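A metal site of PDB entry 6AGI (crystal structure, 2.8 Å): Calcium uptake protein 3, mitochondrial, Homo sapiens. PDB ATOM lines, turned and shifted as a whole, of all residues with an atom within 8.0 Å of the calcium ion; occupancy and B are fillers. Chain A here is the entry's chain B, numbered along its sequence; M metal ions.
The side-chain carboxylate of Glu 126 sits close to the backbone NH of Asp 123, 2.9 Å away. The side-chain carboxylate (OE2) of Glu 126 sits close to the backbone NH (N) of Thr 116, at 2.9 Å. OD2 of Asp 115 sits close to N of Gly 118. The side-chain carboxylate (OD2) of Asp 115 sits at hydrogen-bond distance from the backbone NH (N) of Glu 120 (2.7 Å). OD1 of Asp 117 lies close to OG1 of Thr 116, at 3.5 Å.
Merely in contact with the calcium ion: Asp 123 (3.5 Å). The nearest printed residue that does not touch the calcium ion is Val 122 (4.3 Å).
The calcium ion is bound by the side-chain carboxylate (OE1) of Glu 126. OD1 of Asn 119 is bound to the calcium ion. O of Met 121 binds the calcium ion (2.5 Å). The side-chain carboxylate (OD1) of Asp 115 is bound to the calcium ion, 2.6 Å away. The calcium ion is bound by the side-chain carboxylate (OD1) of Asp 117 (2.8 Å). The calcium ion is bound by OE2 of Glu 126 (2.8 Å). The calcium ion has six donor atoms within binding distance. Slightly farther from the calcium ion lies the side-chain carboxylate (OD2) of Asp 117 (3.0 Å). Slightly farther from the calcium ion lies ND2 of Asn 119 (3.1 Å).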
ATOM      1  N   PHE A 111     -19.405  13.118 -21.988  1.00  0.00           N
ATOM      2  CA  PHE A 111     -20.173  12.393 -20.983  1.00  0.00           C
ATOM      3  C   PHE A 111     -20.433  13.236 -19.734  1.00  0.00           C
ATOM      4  O   PHE A 111     -21.569  13.328 -19.250  1.00  0.00           O
ATOM      5  CB  PHE A 111     -19.449  11.105 -20.590  1.00  0.00           C
ATOM      6  CG  PHE A 111     -20.212  10.266 -19.618  1.00  0.00           C
ATOM      7  CD1 PHE A 111     -21.200   9.401 -20.048  1.00  0.00           C
ATOM      8  CD2 PHE A 111     -19.963  10.369 -18.259  1.00  0.00           C
ATOM      9  CE1 PHE A 111     -21.932   8.631 -19.158  1.00  0.00           C
ATOM     10  CE2 PHE A 111     -20.691   9.600 -17.355  1.00  0.00           C
ATOM     11  CZ  PHE A 111     -21.684   8.734 -17.799  1.00  0.00           C
ATOM     12  N   PHE A 114     -22.891  15.834 -20.126  1.00  0.00           N
ATOM     13  CA  PHE A 114     -24.261  15.328 -20.111  1.00  0.00           C
ATOM     14  C   PHE A 114     -24.772  15.016 -18.706  1.00  0.00           C
ATOM     15  O   PHE A 114     -25.940  15.286 -18.394  1.00  0.00           O
ATOM     16  CB  PHE A 114     -24.347  14.085 -20.988  1.00  0.00           C
ATOM     17  CG  PHE A 114     -24.684  14.347 -22.426  1.00  0.00           C
ATOM     18  CD1 PHE A 114     -25.997  14.581 -22.796  1.00  0.00           C
ATOM     19  CD2 PHE A 114     -23.696  14.332 -23.411  1.00  0.00           C
ATOM     20  CE1 PHE A 114     -26.325  14.808 -24.127  1.00  0.00           C
ATOM     21  CE2 PHE A 114     -24.012  14.565 -24.738  1.00  0.00           C
ATOM     22  CZ  PHE A 114     -25.313  14.806 -25.104  1.00  0.00           C
ATOM     23  N   ASP A 115     -23.931  14.459 -17.836  1.00  0.00           N
ATOM     24  CA  ASP A 115     -24.372  13.931 -16.544  1.00  0.00           C
ATOM     25  C   ASP A 115     -24.521  15.101 -15.567  1.00  0.00           C
ATOM     26  O   ASP A 115     -23.735  15.311 -14.627  1.00  0.00           O
ATOM     27  CB  ASP A 115     -23.401  12.857 -16.060  1.00  0.00           C
ATOM     28  CG  ASP A 115     -23.857  12.138 -14.787  1.00  0.00           C
ATOM     29  OD1 ASP A 115     -25.099  12.058 -14.488  1.00  0.00           O
ATOM     30  OD2 ASP A 115     -22.945  11.578 -14.132  1.00  0.00           O
ATOM     31  N   THR A 116     -25.595  15.854 -15.787  1.00  0.00           N
ATOM     32  CA  THR A 116     -25.966  16.992 -14.952  1.00  0.00           C
ATOM     33  C   THR A 116     -25.904  16.673 -13.446  1.00  0.00           C
ATOM     34  O   THR A 116     -25.571  17.564 -12.663  1.00  0.00           O
ATOM     35  CB  THR A 116     -27.358  17.506 -15.316  1.00  0.00           C
ATOM     36  OG1 THR A 116     -28.330  16.486 -15.044  1.00  0.00           O
ATOM     37  CG2 THR A 116     -27.412  17.825 -16.795  1.00  0.00           C
ATOM     38  N   ASP A 117     -26.226  15.429 -13.026  1.00  0.00           N
ATOM     39  CA  ASP A 117     -26.344  15.105 -11.598  1.00  0.00           C
ATOM     40  C   ASP A 117     -25.226  14.251 -11.009  1.00  0.00           C
ATOM     41  O   ASP A 117     -25.263  13.971  -9.805  1.00  0.00           O
ATOM     42  CB  ASP A 117     -27.663  14.385 -11.277  1.00  0.00           C
ATOM     43  CG  ASP A 117     -27.922  13.213 -12.182  1.00  0.00           C
ATOM     44  OD1 ASP A 117     -28.274  13.434 -13.351  1.00  0.00           O
ATOM     45  OD2 ASP A 117     -27.684  12.063 -11.759  1.00  0.00           O
ATOM     46  N   GLY A 118     -24.307  13.737 -11.795  1.00  0.00           N
ATOM     47  CA  GLY A 118     -23.144  13.107 -11.200  1.00  0.00           C
ATOM     48  C   GLY A 118     -23.288  11.635 -10.844  1.00  0.00           C
ATOM     49  O   GLY A 118     -22.319  11.050 -10.346  1.00  0.00           O
ATOM     50  N   ASN A 119     -24.445  11.026 -11.080  1.00  0.00           N
ATOM     51  CA  ASN A 119     -24.559   9.595 -10.806  1.00  0.00           C
ATOM     52  C   ASN A 119     -23.754   8.719 -11.769  1.00  0.00           C
ATOM     53  O   ASN A 119     -23.785   7.510 -11.606  1.00  0.00           O
ATOM     54  CB  ASN A 119     -26.023   9.158 -10.873  1.00  0.00           C
ATOM     55  CG  ASN A 119     -26.622   9.376 -12.233  1.00  0.00           C
ATOM     56  OD1 ASN A 119     -25.936   9.850 -13.157  1.00  0.00           O
ATOM     57  ND2 ASN A 119     -27.905   9.050 -12.375  1.00  0.00           N
ATOM     58  N   GLU A 120     -23.113   9.287 -12.789  1.00  0.00           N
ATOM     59  CA  GLU A 120     -22.325   8.525 -13.760  1.00  0.00           C
ATOM     60  C   GLU A 120     -23.163   7.665 -14.694  1.00  0.00           C
ATOM     61  O   GLU A 120     -22.651   6.719 -15.304  1.00  0.00           O
ATOM     62  CB  GLU A 120     -21.258   7.687 -13.066  1.00  0.00           C
ATOM     63  CG  GLU A 120     -20.103   8.544 -12.775  1.00  0.00           C
ATOM     64  CD  GLU A 120     -19.433   8.138 -11.528  1.00  0.00           C
ATOM     65  OE1 GLU A 120     -19.804   7.095 -10.957  1.00  0.00           O
ATOM     66  OE2 GLU A 120     -18.599   8.940 -11.082  1.00  0.00           O
ATOM     67  N   MET A 121     -24.450   7.948 -14.812  1.00  0.00           N
ATOM     68  CA  MET A 121     -25.220   7.446 -15.931  1.00  0.00           C
ATOM     69  C   MET A 121     -25.873   8.659 -16.597  1.00  0.00           C
ATOM     70  O   MET A 121     -25.908   9.752 -16.025  1.00  0.00           O
ATOM     71  CB  MET A 121     -26.297   6.381 -15.546  1.00  0.00           C
ATOM     72  CG  MET A 121     -25.927   5.246 -14.550  1.00  0.00           C
ATOM     73  SD  MET A 121     -24.625   4.133 -15.179  1.00  0.00           S
ATOM     74  CE  MET A 121     -25.507   2.604 -15.495  1.00  0.00           C
ATOM     75  N   VAL A 122     -26.382   8.463 -17.798  1.00  0.00           N
ATOM     76  CA  VAL A 122     -27.075   9.516 -18.535  1.00  0.00           C
ATOM     77  C   VAL A 122     -28.476   8.989 -18.829  1.00  0.00           C
ATOM     78  O   VAL A 122     -28.646   7.977 -19.500  1.00  0.00           O
ATOM     79  CB  VAL A 122     -26.335   9.923 -19.823  1.00  0.00           C
ATOM     80  CG1 VAL A 122     -27.172  10.841 -20.667  1.00  0.00           C
ATOM     81  CG2 VAL A 122     -25.080  10.662 -19.460  1.00  0.00           C
ATOM     82  N   ASP A 123     -29.472   9.641 -18.217  1.00  0.00           N
ATOM     83  CA  ASP A 123     -30.889   9.413 -18.473  1.00  0.00           C
ATOM     84  C   ASP A 123     -31.234   9.754 -19.915  1.00  0.00           C
ATOM     85  O   ASP A 123     -30.531  10.504 -20.583  1.00  0.00           O
ATOM     86  CB  ASP A 123     -31.748  10.314 -17.589  1.00  0.00           C
ATOM     87  CG  ASP A 123     -31.301  10.322 -16.143  1.00  0.00           C
ATOM     88  OD1 ASP A 123     -30.385   9.548 -15.787  1.00  0.00           O
ATOM     89  OD2 ASP A 123     -31.834  11.157 -15.380  1.00  0.00           O
ATOM     90  N   LYS A 124     -32.361   9.221 -20.373  1.00  0.00           N
ATOM     91  CA  LYS A 124     -32.989   9.766 -21.572  1.00  0.00           C
ATOM     92  C   LYS A 124     -33.283  11.254 -21.405  1.00  0.00           C
ATOM     93  O   LYS A 124     -33.229  12.000 -22.386  1.00  0.00           O
ATOM     94  CB  LYS A 124     -34.275   9.001 -21.896  1.00  0.00           C
ATOM     95  CG  LYS A 124     -34.940   9.364 -23.220  1.00  0.00           C
ATOM     96  CD  LYS A 124     -36.137   8.446 -23.433  1.00  0.00           C
ATOM     97  CE  LYS A 124     -37.101   8.895 -24.518  1.00  0.00           C
ATOM     98  NZ  LYS A 124     -38.125   7.813 -24.681  1.00  0.00           N
ATOM     99  N   LYS A 125     -33.583  11.695 -20.186  1.00  0.00           N
ATOM    100  CA  LYS A 125     -34.050  13.064 -19.983  1.00  0.00           C
ATOM    101  C   LYS A 125     -32.867  14.032 -19.965  1.00  0.00           C
ATOM    102  O   LYS A 125     -32.923  15.103 -20.606  1.00  0.00           O
ATOM    103  CB  LYS A 125     -34.841  13.119 -18.665  1.00  0.00           C
ATOM    104  CG  LYS A 125     -35.315  14.488 -18.209  1.00  0.00           C
ATOM    105  CD  LYS A 125     -34.914  14.761 -16.753  1.00  0.00           C
ATOM    106  CE  LYS A 125     -33.576  15.474 -16.630  1.00  0.00           C
ATOM    107  NZ  LYS A 125     -32.965  15.326 -15.273  1.00  0.00           N
ATOM    108  N   GLU A 126     -31.760  13.596 -19.344  1.00  0.00           N
ATOM    109  CA  GLU A 126     -30.473  14.276 -19.523  1.00  0.00           C
ATOM    110  C   GLU A 126     -30.105  14.397 -20.992  1.00  0.00           C
ATOM    111  O   GLU A 126     -29.780  15.492 -21.481  1.00  0.00           O
ATOM    112  CB  GLU A 126     -29.365  13.536 -18.781  1.00  0.00           C
ATOM    113  CG  GLU A 126     -29.208  13.969 -17.361  1.00  0.00           C
ATOM    114  CD  GLU A 126     -28.245  13.095 -16.591  1.00  0.00           C
ATOM    115  OE1 GLU A 126     -28.222  11.876 -16.836  1.00  0.00           O
ATOM    116  OE2 GLU A 126     -27.487  13.625 -15.764  1.00  0.00           O
ATOM    117  N   PHE A 127     -30.161  13.287 -21.721  1.00  0.00           N
ATOM    118  CA  PHE A 127     -29.798  13.317 -23.122  1.00  0.00           C
ATOM    119  C   PHE A 127     -30.708  14.252 -23.899  1.00  0.00           C
ATOM    120  O   PHE A 127     -30.279  14.824 -24.892  1.00  0.00           O
ATOM    121  CB  PHE A 127     -29.830  11.901 -23.722  1.00  0.00           C
ATOM    122  CG  PHE A 127     -29.277  11.829 -25.101  1.00  0.00           C
ATOM    123  CD1 PHE A 127     -30.088  12.002 -26.221  1.00  0.00           C
ATOM    124  CD2 PHE A 127     -27.913  11.656 -25.300  1.00  0.00           C
ATOM    125  CE1 PHE A 127     -29.554  11.945 -27.490  1.00  0.00           C
ATOM    126  CE2 PHE A 127     -27.371  11.620 -26.579  1.00  0.00           C
ATOM    127  CZ  PHE A 127     -28.206  11.758 -27.670  1.00  0.00           C
ATOM    128  N   GLU A 224     -30.265   3.336 -18.904  1.00  0.00           N
ATOM    129  CA  GLU A 224     -29.301   4.407 -18.692  1.00  0.00           C
ATOM    130  C   GLU A 224     -27.939   4.035 -19.248  1.00  0.00           C
ATOM    131  O   GLU A 224     -27.617   2.865 -19.442  1.00  0.00           O
ATOM    132  CB  GLU A 224     -29.157   4.764 -17.202  1.00  0.00           C
ATOM    133  CG  GLU A 224     -30.429   5.224 -16.503  1.00  0.00           C
ATOM    134  CD  GLU A 224     -30.828   4.275 -15.383  1.00  0.00           C
ATOM    135  OE1 GLU A 224     -29.963   3.469 -14.946  1.00  0.00           O
ATOM    136  OE2 GLU A 224     -31.997   4.327 -14.934  1.00  0.00           O
ATOM    137  N   LEU A 225     -27.144   5.093 -19.525  1.00  0.00           N
ATOM    138  CA  LEU A 225     -25.879   5.008 -20.240  1.00  0.00           C
ATOM    139  C   LEU A 225     -24.733   5.342 -19.303  1.00  0.00           C
ATOM    140  O   LEU A 225     -24.687   6.431 -18.741  1.00  0.00           O
ATOM    141  CB  LEU A 225     -25.871   5.983 -21.411  1.00  0.00           C
ATOM    142  CG  LEU A 225     -26.340   5.557 -22.790  1.00  0.00           C
ATOM    143  CD1 LEU A 225     -26.025   6.716 -23.741  1.00  0.00           C
ATOM    144  CD2 LEU A 225     -25.611   4.303 -23.218  1.00  0.00           C
HETATM  145 CA    CA M   1     -27.503  11.100 -14.603  1.00  0.00          CA
